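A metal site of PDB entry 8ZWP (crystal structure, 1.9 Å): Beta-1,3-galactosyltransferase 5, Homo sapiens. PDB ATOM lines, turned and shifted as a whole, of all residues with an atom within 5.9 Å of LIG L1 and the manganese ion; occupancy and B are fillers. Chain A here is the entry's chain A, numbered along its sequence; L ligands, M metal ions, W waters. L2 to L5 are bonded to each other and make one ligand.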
ATOM      1  N   VAL A  33      -7.655  14.879  16.796  1.00  0.00           N
ATOM      2  CA  VAL A  33      -8.750  15.012  15.834  1.00  0.00           C
ATOM      3  C   VAL A  33      -8.164  15.090  14.430  1.00  0.00           C
ATOM      4  O   VAL A  33      -7.331  15.952  14.150  1.00  0.00           O
ATOM      5  CB  VAL A  33      -9.595  16.271  16.125  1.00  0.00           C
ATOM      6  CG1 VAL A  33     -10.730  16.384  15.081  1.00  0.00           C
ATOM      7  CG2 VAL A  33     -10.127  16.251  17.553  1.00  0.00           C
ATOM      8  N   THR A  34      -8.615  14.207  13.547  1.00  0.00           N
ATOM      9  CA  THR A  34      -8.213  14.275  12.154  1.00  0.00           C
ATOM     10  C   THR A  34      -9.140  15.200  11.368  1.00  0.00           C
ATOM     11  O   THR A  34     -10.367  15.200  11.569  1.00  0.00           O
ATOM     12  CB  THR A  34      -8.211  12.884  11.508  1.00  0.00           C
ATOM     13  OG1 THR A  34      -9.539  12.357  11.550  1.00  0.00           O
ATOM     14  CG2 THR A  34      -7.254  11.959  12.259  1.00  0.00           C
ATOM     15  N   SER A  35      -8.545  16.018  10.499  1.00  0.00           N
ATOM     16  CA  SER A  35      -9.307  16.849   9.585  1.00  0.00           C
ATOM     17  C   SER A  35      -8.358  17.301   8.481  1.00  0.00           C
ATOM     18  O   SER A  35      -7.144  17.331   8.666  1.00  0.00           O
ATOM     19  CB  SER A  35      -9.943  18.061  10.297  1.00  0.00           C
ATOM     20  OG  SER A  35      -8.959  18.964  10.773  1.00  0.00           O
ATOM     21  N   SER A  36      -8.931  17.639   7.325  1.00  0.00           N
ATOM     22  CA  SER A  36      -8.116  18.134   6.227  1.00  0.00           C
ATOM     23  C   SER A  36      -7.934  19.655   6.356  1.00  0.00           C
ATOM     24  O   SER A  36      -8.607  20.306   7.158  1.00  0.00           O
ATOM     25  CB  SER A  36      -8.722  17.727   4.888  1.00  0.00           C
ATOM     26  OG  SER A  36      -9.915  18.425   4.615  1.00  0.00           O
ATOM     27  N   GLN A  39     -10.940  22.043   6.210  1.00  0.00           N
ATOM     28  CA  GLN A  39     -12.002  21.836   7.198  1.00  0.00           C
ATOM     29  C   GLN A  39     -11.833  22.715   8.434  1.00  0.00           C
ATOM     30  O   GLN A  39     -11.996  22.238   9.556  1.00  0.00           O
ATOM     31  CB  GLN A  39     -12.087  20.364   7.578  1.00  0.00           C
ATOM     32  CG  GLN A  39     -12.523  19.474   6.428  1.00  0.00           C
ATOM     33  CD  GLN A  39     -12.743  18.039   6.836  1.00  0.00           C
ATOM     34  OE1 GLN A  39     -11.794  17.319   7.142  1.00  0.00           O
ATOM     35  NE2 GLN A  39     -13.996  17.585   6.805  1.00  0.00           N
ATOM     36  N   LEU A  66      -4.639  16.910  14.022  1.00  0.00           N
ATOM     37  CA  LEU A  66      -3.597  16.254  13.232  1.00  0.00           C
ATOM     38  C   LEU A  66      -3.682  16.726  11.784  1.00  0.00           C
ATOM     39  O   LEU A  66      -4.738  16.581  11.149  1.00  0.00           O
ATOM     40  CB  LEU A  66      -3.766  14.738  13.315  1.00  0.00           C
ATOM     41  CG  LEU A  66      -3.830  14.136  14.712  1.00  0.00           C
ATOM     42  CD1 LEU A  66      -4.042  12.625  14.669  1.00  0.00           C
ATOM     43  CD2 LEU A  66      -2.529  14.450  15.480  1.00  0.00           C
ATOM     44  N   ASP A  96      -1.500  15.331   2.831  1.00  0.00           N
ATOM     45  CA  ASP A  96      -2.705  15.082   3.614  1.00  0.00           C
ATOM     46  C   ASP A  96      -3.874  14.749   2.684  1.00  0.00           C
ATOM     47  O   ASP A  96      -4.571  15.625   2.193  1.00  0.00           O
ATOM     48  CB  ASP A  96      -2.987  16.294   4.492  1.00  0.00           C
ATOM     49  CG  ASP A  96      -3.986  15.990   5.595  1.00  0.00           C
ATOM     50  OD1 ASP A  96      -4.735  14.998   5.449  1.00  0.00           O
ATOM     51  OD2 ASP A  96      -3.986  16.732   6.602  1.00  0.00           O
ATOM     52  N   VAL A  97      -4.072  13.444   2.418  1.00  0.00           N
ATOM     53  CA  VAL A  97      -5.182  12.960   1.601  1.00  0.00           C
ATOM     54  C   VAL A  97      -5.779  11.712   2.250  1.00  0.00           C
ATOM     55  O   VAL A  97      -5.159  11.098   3.118  1.00  0.00           O
ATOM     56  CB  VAL A  97      -4.743  12.616   0.163  1.00  0.00           C
ATOM     57  CG1 VAL A  97      -4.300  13.865  -0.563  1.00  0.00           C
ATOM     58  CG2 VAL A  97      -3.634  11.572   0.210  1.00  0.00           C
ATOM     59  N   TYR A  98      -6.989  11.333   1.814  1.00  0.00           N
ATOM     60  CA  TYR A  98      -7.683  10.241   2.500  1.00  0.00           C
ATOM     61  C   TYR A  98      -6.796   8.995   2.579  1.00  0.00           C
ATOM     62  O   TYR A  98      -6.679   8.371   3.643  1.00  0.00           O
ATOM     63  CB  TYR A  98      -9.026   9.890   1.836  1.00  0.00           C
ATOM     64  CG  TYR A  98      -9.885   8.989   2.729  1.00  0.00           C
ATOM     65  CD1 TYR A  98      -9.795   7.596   2.651  1.00  0.00           C
ATOM     66  CD2 TYR A  98     -10.768   9.531   3.661  1.00  0.00           C
ATOM     67  CE1 TYR A  98     -10.570   6.763   3.470  1.00  0.00           C
ATOM     68  CE2 TYR A  98     -11.549   8.705   4.500  1.00  0.00           C
ATOM     69  CZ  TYR A  98     -11.432   7.327   4.396  1.00  0.00           C
ATOM     70  OH  TYR A  98     -12.183   6.502   5.199  1.00  0.00           O
ATOM     71  N   LEU A 101      -4.314   8.553   5.520  1.00  0.00           N
ATOM     72  CA  LEU A 101      -4.767   8.610   6.905  1.00  0.00           C
ATOM     73  C   LEU A 101      -3.946   7.734   7.845  1.00  0.00           C
ATOM     74  O   LEU A 101      -3.820   8.045   9.020  1.00  0.00           O
ATOM     75  CB  LEU A 101      -6.256   8.230   6.953  1.00  0.00           C
ATOM     76  CG  LEU A 101      -7.105   9.402   6.500  1.00  0.00           C
ATOM     77  CD1 LEU A 101      -8.606   9.007   6.502  1.00  0.00           C
ATOM     78  CD2 LEU A 101      -6.852  10.629   7.381  1.00  0.00           C
ATOM     79  N   LYS A 104      -1.259   9.781   9.067  1.00  0.00           N
ATOM     80  CA  LYS A 104      -1.779  10.779   9.992  1.00  0.00           C
ATOM     81  C   LYS A 104      -1.949  10.169  11.378  1.00  0.00           C
ATOM     82  O   LYS A 104      -1.505  10.743  12.384  1.00  0.00           O
ATOM     83  CB  LYS A 104      -3.100  11.355   9.490  1.00  0.00           C
ATOM     84  CG  LYS A 104      -3.609  12.468  10.399  1.00  0.00           C
ATOM     85  CD  LYS A 104      -4.776  13.240   9.784  1.00  0.00           C
ATOM     86  CE  LYS A 104      -4.305  14.153   8.647  1.00  0.00           C
ATOM     87  NZ  LYS A 104      -5.323  15.226   8.357  1.00  0.00           N
ATOM     88  N   THR A 125     -10.047  10.654  16.904  1.00  0.00           N
ATOM     89  CA  THR A 125     -11.411  10.827  16.431  1.00  0.00           C
ATOM     90  C   THR A 125     -11.475  11.585  15.106  1.00  0.00           C
ATOM     91  O   THR A 125     -10.597  12.392  14.774  1.00  0.00           O
ATOM     92  CB  THR A 125     -12.292  11.523  17.506  1.00  0.00           C
ATOM     93  OG1 THR A 125     -13.663  11.517  17.078  1.00  0.00           O
ATOM     94  CG2 THR A 125     -11.838  12.960  17.754  1.00  0.00           C
ATOM     95  N   ASP A 126     -12.541  11.309  14.356  1.00  0.00           N
ATOM     96  CA  ASP A 126     -12.936  12.052  13.169  1.00  0.00           C
ATOM     97  C   ASP A 126     -13.406  13.456  13.563  1.00  0.00           C
ATOM     98  O   ASP A 126     -13.733  13.743  14.714  1.00  0.00           O
ATOM     99  CB  ASP A 126     -14.110  11.379  12.438  1.00  0.00           C
ATOM    100  CG  ASP A 126     -13.723  10.347  11.366  1.00  0.00           C
ATOM    101  OD1 ASP A 126     -12.644   9.735  11.412  1.00  0.00           O
ATOM    102  OD2 ASP A 126     -14.585  10.129  10.453  1.00  0.00           O
ATOM    103  N   SER A 127     -13.533  14.315  12.572  1.00  0.00           N
ATOM    104  CA  SER A 127     -13.990  15.677  12.847  1.00  0.00           C
ATOM    105  C   SER A 127     -15.507  15.831  12.739  1.00  0.00           C
ATOM    106  O   SER A 127     -16.061  16.790  13.287  1.00  0.00           O
ATOM    107  CB  SER A 127     -13.289  16.671  11.927  1.00  0.00           C
ATOM    108  OG  SER A 127     -13.421  16.248  10.574  1.00  0.00           O
ATOM    109  N   ASP A 128     -16.186  14.934  12.017  1.00  0.00           N
ATOM    110  CA  ASP A 128     -17.652  15.014  11.890  1.00  0.00           C
ATOM    111  C   ASP A 128     -18.307  14.186  13.005  1.00  0.00           C
ATOM    112  O   ASP A 128     -19.099  13.278  12.784  1.00  0.00           O
ATOM    113  CB  ASP A 128     -18.099  14.598  10.495  1.00  0.00           C
ATOM    114  CG  ASP A 128     -17.598  13.218  10.073  1.00  0.00           C
ATOM    115  OD1 ASP A 128     -16.579  12.732  10.582  1.00  0.00           O
ATOM    116  OD2 ASP A 128     -18.229  12.631   9.170  1.00  0.00           O
ATOM    117  N   MET A 129     -17.967  14.575  14.237  1.00  0.00           N
ATOM    118  CA  MET A 129     -18.303  13.787  15.417  1.00  0.00           C
ATOM    119  C   MET A 129     -18.847  14.678  16.534  1.00  0.00           C
ATOM    120  O   MET A 129     -18.434  15.831  16.673  1.00  0.00           O
ATOM    121  CB  MET A 129     -17.070  13.066  15.994  1.00  0.00           C
ATOM    122  CG  MET A 129     -16.453  12.012  15.080  1.00  0.00           C
ATOM    123  SD  MET A 129     -17.414  10.510  14.924  1.00  0.00           S
ATOM    124  CE  MET A 129     -17.283   9.844  16.573  1.00  0.00           C
ATOM    125  N   LYS A 167     -15.082   3.289  -1.475  1.00  0.00           N
ATOM    126  CA  LYS A 167     -14.121   4.126  -0.772  1.00  0.00           C
ATOM    127  C   LYS A 167     -13.111   3.314   0.047  1.00  0.00           C
ATOM    128  O   LYS A 167     -11.950   3.721   0.181  1.00  0.00           O
ATOM    129  CB  LYS A 167     -14.897   5.086   0.139  1.00  0.00           C
ATOM    130  CG  LYS A 167     -14.053   5.965   1.040  1.00  0.00           C
ATOM    131  CD  LYS A 167     -14.967   6.702   2.023  1.00  0.00           C
ATOM    132  CE  LYS A 167     -14.212   7.731   2.848  1.00  0.00           C
ATOM    133  NZ  LYS A 167     -13.731   8.890   2.045  1.00  0.00           N
ATOM    134  N   TRP A 168     -13.527   2.164   0.552  1.00  0.00           N
ATOM    135  CA  TRP A 168     -12.679   1.319   1.382  1.00  0.00           C
ATOM    136  C   TRP A 168     -12.157   0.088   0.640  1.00  0.00           C
ATOM    137  O   TRP A 168     -11.786  -0.907   1.271  1.00  0.00           O
ATOM    138  CB  TRP A 168     -13.441   0.921   2.632  1.00  0.00           C
ATOM    139  CG  TRP A 168     -13.842   2.104   3.473  1.00  0.00           C
ATOM    140  CD1 TRP A 168     -13.047   3.162   3.878  1.00  0.00           C
ATOM    141  CD2 TRP A 168     -15.141   2.372   3.978  1.00  0.00           C
ATOM    142  NE1 TRP A 168     -13.786   4.048   4.629  1.00  0.00           N
ATOM    143  CE2 TRP A 168     -15.076   3.590   4.707  1.00  0.00           C
ATOM    144  CE3 TRP A 168     -16.365   1.694   3.910  1.00  0.00           C
ATOM    145  CZ2 TRP A 168     -16.189   4.135   5.339  1.00  0.00           C
ATOM    146  CZ3 TRP A 168     -17.459   2.231   4.551  1.00  0.00           C
ATOM    147  CH2 TRP A 168     -17.365   3.441   5.256  1.00  0.00           C
ATOM    148  N   THR A 187     -13.767   6.099  13.309  1.00  0.00           N
ATOM    149  CA  THR A 187     -14.508   7.307  13.650  1.00  0.00           C
ATOM    150  C   THR A 187     -14.133   7.826  15.043  1.00  0.00           C
ATOM    151  O   THR A 187     -14.196   9.038  15.293  1.00  0.00           O
ATOM    152  CB  THR A 187     -16.025   7.079  13.551  1.00  0.00           C
ATOM    153  OG1 THR A 187     -16.439   5.983  14.375  1.00  0.00           O
ATOM    154  CG2 THR A 187     -16.440   6.834  12.078  1.00  0.00           C
ATOM    155  N   HIS A 255     -21.229   9.760  15.137  1.00  0.00           N
ATOM    156  CA  HIS A 255     -20.687  10.154  13.842  1.00  0.00           C
ATOM    157  C   HIS A 255     -21.748  10.870  12.992  1.00  0.00           C
ATOM    158  O   HIS A 255     -22.925  10.960  13.358  1.00  0.00           O
ATOM    159  CB  HIS A 255     -20.142   8.890  13.162  1.00  0.00           C
ATOM    160  CG  HIS A 255     -19.370   9.110  11.893  1.00  0.00           C
ATOM    161  ND1 HIS A 255     -19.508   8.240  10.823  1.00  0.00           N
ATOM    162  CD2 HIS A 255     -18.414   9.987  11.539  1.00  0.00           C
ATOM    163  CE1 HIS A 255     -18.705   8.620   9.845  1.00  0.00           C
ATOM    164  NE2 HIS A 255     -18.017   9.663  10.260  1.00  0.00           N
ATOM    165  N   PHE A 256     -21.310  11.365  11.834  1.00  0.00           N
ATOM    166  CA  PHE A 256     -22.216  11.967  10.851  1.00  0.00           C
ATOM    167  C   PHE A 256     -22.799  13.281  11.357  1.00  0.00           C
ATOM    168  O   PHE A 256     -23.977  13.568  11.155  1.00  0.00           O
ATOM    169  CB  PHE A 256     -23.334  11.002  10.466  1.00  0.00           C
ATOM    170  CG  PHE A 256     -22.856   9.810   9.655  1.00  0.00           C
ATOM    171  CD1 PHE A 256     -21.950  10.004   8.623  1.00  0.00           C
ATOM    172  CD2 PHE A 256     -23.265   8.533   9.951  1.00  0.00           C
ATOM    173  CE1 PHE A 256     -21.507   8.931   7.863  1.00  0.00           C
ATOM    174  CE2 PHE A 256     -22.815   7.433   9.183  1.00  0.00           C
ATOM    175  CZ  PHE A 256     -21.941   7.653   8.152  1.00  0.00           C
HETATM  176  N1  LIG L   1      -9.533  13.496   6.710  1.00  0.00           N
HETATM  177  C1  LIG L   1      -8.273  14.084   6.804  1.00  0.00           C
HETATM  178  N2  LIG L   1      -7.645  14.319   5.597  1.00  0.00           N
HETATM  179  C2  LIG L   1      -8.155  14.018   4.341  1.00  0.00           C
HETATM  180  C3  LIG L   1      -9.446  13.418   4.335  1.00  0.00           C
HETATM  181  C4  LIG L   1     -10.091  13.182   5.494  1.00  0.00           C
HETATM  182  O1  LIG L   1      -7.739  14.379   7.873  1.00  0.00           O
HETATM  183  O2  LIG L   1      -7.480  14.284   3.337  1.00  0.00           O
HETATM  184  C5  LIG L   1     -10.276  13.224   7.961  1.00  0.00           C
HETATM  185  C6  LIG L   1     -11.695  13.780   7.947  1.00  0.00           C
HETATM  186  O3  LIG L   1     -11.784  15.131   8.367  1.00  0.00           O
HETATM  187  C7  LIG L   1     -12.366  12.849   8.966  1.00  0.00           C
HETATM  188  C8  LIG L   1     -11.698  11.506   8.675  1.00  0.00           C
HETATM  189  O4  LIG L   1     -10.411  11.813   8.086  1.00  0.00           O
HETATM  190  O5  LIG L   1     -12.090  13.297  10.282  1.00  0.00           O
HETATM  191  C9  LIG L   1     -12.466  10.607   7.743  1.00  0.00           C
HETATM  192  O6  LIG L   1     -12.945  11.393   6.625  1.00  0.00           O
HETATM  193  P1  LIG L   1     -14.492  11.484   6.306  1.00  0.00           P
HETATM  194  O7  LIG L   1     -14.640  12.381   5.129  1.00  0.00           O
HETATM  195  O8  LIG L   1     -15.283  11.879   7.559  1.00  0.00           O
HETATM  196  O9  LIG L   1     -14.913   9.981   5.928  1.00  0.00           O
HETATM  197  P2  LIG L   1     -16.277   9.271   6.306  1.00  0.00           P
HETATM  198  O10 LIG L   1     -17.300  10.000   5.438  1.00  0.00           O
HETATM  199  O11 LIG L   1     -16.089   7.849   5.777  1.00  0.00           O
HETATM  200  O12 LIG L   1     -16.591   9.385   7.794  1.00  0.00           O
HETATM  201  C1  LG2 L   2     -21.428   3.877  -0.695  1.00  0.00           C
HETATM  202  C2  LG2 L   2     -20.953   2.856   0.321  1.00  0.00           C
HETATM  203  C3  LG2 L   2     -20.169   3.527   1.443  1.00  0.00           C
HETATM  204  C4  LG2 L   2     -20.956   4.708   2.031  1.00  0.00           C
HETATM  205  C5  LG2 L   2     -20.132   5.532   3.004  1.00  0.00           C
HETATM  206  C6  LG2 L   2     -22.202   4.994   0.001  1.00  0.00           C
HETATM  207  O1  LG2 L   2     -22.581   5.948  -0.951  1.00  0.00           O
HETATM  208  O2  LG2 L   2     -22.265   3.250  -1.671  1.00  0.00           O
HETATM  209  O3  LG2 L   2     -20.156   1.863  -0.323  1.00  0.00           O
HETATM  210  O4  LG2 L   2     -19.837   2.600   2.471  1.00  0.00           O
HETATM  211  O5  LG2 L   2     -21.372   5.604   0.991  1.00  0.00           O
HETATM  212  O6  LG2 L   2     -19.439   6.571   2.335  1.00  0.00           O
HETATM  213  C1  LG3 L   3     -20.967   1.946   3.110  1.00  0.00           C
HETATM  214  C2  LG3 L   3     -20.645   0.438   3.122  1.00  0.00           C
HETATM  215  C3  LG3 L   3     -21.665  -0.379   3.887  1.00  0.00           C
HETATM  216  C4  LG3 L   3     -21.648   0.115   5.311  1.00  0.00           C
HETATM  217  C5  LG3 L   3     -21.977   1.624   5.341  1.00  0.00           C
HETATM  218  C6  LG3 L   3     -21.814   2.274   6.762  1.00  0.00           C
HETATM  219  O1  LG3 L   3     -20.573  -0.100   1.801  1.00  0.00           O
HETATM  220  O2  LG3 L   3     -21.309  -1.777   3.909  1.00  0.00           O
HETATM  221  O3  LG3 L   3     -20.325  -0.067   5.863  1.00  0.00           O
HETATM  222  O4  LG3 L   3     -21.207   2.463   4.430  1.00  0.00           O
HETATM  223  O5  LG3 L   3     -20.796   3.262   6.813  1.00  0.00           O
HETATM  224  C1  LG4 L   4     -20.252  -0.869   7.050  1.00  0.00           C
HETATM  225  C2  LG4 L   4     -19.144  -0.313   7.940  1.00  0.00           C
HETATM  226  C3  LG4 L   4     -17.788  -0.560   7.341  1.00  0.00           C
HETATM  227  C4  LG4 L   4     -17.631  -2.033   7.089  1.00  0.00           C
HETATM  228  C5  LG4 L   4     -18.703  -2.573   6.150  1.00  0.00           C
HETATM  229  C6  LG4 L   4     -18.602  -4.059   5.971  1.00  0.00           C
HETATM  230  O1  LG4 L   4     -19.301   1.109   8.106  1.00  0.00           O
HETATM  231  O2  LG4 L   4     -16.750  -0.124   8.247  1.00  0.00           O
HETATM  232  O3  LG4 L   4     -17.810  -2.701   8.340  1.00  0.00           O
HETATM  233  O4  LG4 L   4     -20.056  -2.312   6.706  1.00  0.00           O
HETATM  234  O5  LG4 L   4     -19.603  -4.439   5.040  1.00  0.00           O
HETATM  235  C1  LG5 L   5     -15.599   0.382   7.543  1.00  0.00           C
HETATM  236  C2  LG5 L   5     -14.934   1.450   8.397  1.00  0.00           C
HETATM  237  C3  LG5 L   5     -13.667   1.937   7.706  1.00  0.00           C
HETATM  238  C4  LG5 L   5     -12.755   0.769   7.301  1.00  0.00           C
HETATM  239  C5  LG5 L   5     -13.574  -0.264   6.528  1.00  0.00           C
HETATM  240  C6  LG5 L   5     -12.752  -1.506   6.158  1.00  0.00           C
HETATM  241  C7  LG5 L   5     -16.455   2.824   9.785  1.00  0.00           C
HETATM  242  C8  LG5 L   5     -17.695   3.695   9.742  1.00  0.00           C
HETATM  243  N1  LG5 L   5     -15.831   2.595   8.619  1.00  0.00           N
HETATM  244  O1  LG5 L   5     -12.940   2.838   8.552  1.00  0.00           O
HETATM  245  O2  LG5 L   5     -12.147   0.170   8.424  1.00  0.00           O
HETATM  246  O3  LG5 L   5     -14.689  -0.686   7.288  1.00  0.00           O
HETATM  247  O4  LG5 L   5     -13.552  -2.306   5.300  1.00  0.00           O
HETATM  248  O5  LG5 L   5     -16.068   2.400  10.860  1.00  0.00           O
HETATM  249 MN    MN M   1     -16.416  10.864   9.216  1.00  0.00          MN
HETATM  250  O   HOH W   1     -18.980  11.702   6.625  1.00  0.00           O
HETATM  251  O   HOH W   2     -13.451   7.589   7.197  1.00  0.00           O
HETATM  252  O   HOH W   3      -7.465  16.281   1.745  1.00  0.00           O
HETATM  253  O   HOH W   4     -13.621  14.719   5.044  1.00  0.00           O
HETATM  254  O   HOH W   5     -16.458  14.117   7.019  1.00  0.00           O
HETATM  255  O   HOH W   6     -16.614   6.419   8.196  1.00  0.00           O
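Within 4 Å of the manganese ion: Asp 126, Asp 128 and His 255.
The manganese ion is bound by an oxygen (O12) of LIG L1 (2.1 Å), an oxygen (O8) of LIG L1 (2.2 Å), a ring nitrogen (NE2) of His 255 (2.3 Å), the side-chain carboxylate (OD1) of Asp 128 (2.3 Å), the side-chain carboxylate (OD2) of Asp 126 (2.3 Å) and the side-chain carboxylate (OD2) of Asp 128 (2.5 Å).
Water W4 bridges O7 of LIG L1 and NE2 of Gln 39.
Water W3 bridges an oxygen (O2) of LIG L1 (2.6 Å) and the backbone carbonyl oxygen of Asp 96 (3.0 Å).
Water W2 bridges OH of Tyr 98 (2.6 Å) and O11 of LIG L1 (3.0 Å).
O of Thr 187 lies within hydrogen-bond range of N of Asp 126 (3.0 Å).
The backbone NH of Ser 36 sits at hydrogen-bond distance from the side-chain amide oxygen of Gln 39, at 2.9 Å.
OD2 of Asp 96 is in salt-bridge range of NZ of Lys 104.
O of Ser 35 sits at hydrogen-bond distance from NZ of Lys 104 (2.8 Å).
The backbone carbonyl oxygen (O) of Leu 66 is in hydrogen-bond range of the side-chain amino group (NZ) of Lys 104.
The backbone carbonyl oxygen of Thr 34 lies close to the side-chain hydroxyl of Ser 127.
The backbone carbonyl oxygen of Thr 125 sits at hydrogen-bond distance from the backbone NH of Thr 34.
The side-chain hydroxyl of Tyr 98 sits at hydrogen-bond distance from the indole nitrogen of Trp 168, 3.0 Å away.
Ser 36 touches LIG L1.
Val 97 touches LIG L1.
Leu 101 touches LIG L1 (CD1 to O4, 3.7 Å).
Lys 167 touches LIG L1.
Trp 168 touches LIG L1.
Hydrophobic or aromatic side chains that line LIG L1: Tyr 98, Leu 101, Trp 168 and His 255.
15 residues have an atom within 4 Å of LIG L1: Thr 34, Ser 35, Ser 36, Gln 39, Asp 96, Val 97, Tyr 98, Leu 101, Lys 104, Asp 126, Ser 127, Asp 128, Lys 167, Trp 168 and His 255.
The side-chain amide oxygen (OE1) of Gln 39 lies within hydrogen-bond range of an oxygen (O3) of LIG L1 (2.5 Å).
NZ of Lys 104 sits at hydrogen-bond distance from O1 of LIG L1, at 2.6 Å.
The backbone carbonyl oxygen (O) of Thr 34 is in hydrogen-bond range of an oxygen (O5) of LIG L1 (2.9 Å).
OG1 of Thr 34 lies within hydrogen-bond range of O5 of LIG L1, at 3.0 Å.
N of Ser 127 sits at hydrogen-bond distance from O5 of LIG L1.
The side-chain hydroxyl of Ser 127 lies within hydrogen-bond range of an oxygen (O3) of LIG L1 (3.0 Å).
N2 of LIG L1 lies within hydrogen-bond range of OD1 of Asp 96 (3.0 Å).
O1 of LIG L1 sits close to N of Ser 35, 3.2 Å away.
O2 of LIG L1 lies within hydrogen-bond range of N of Tyr 98, 3.4 Å away.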
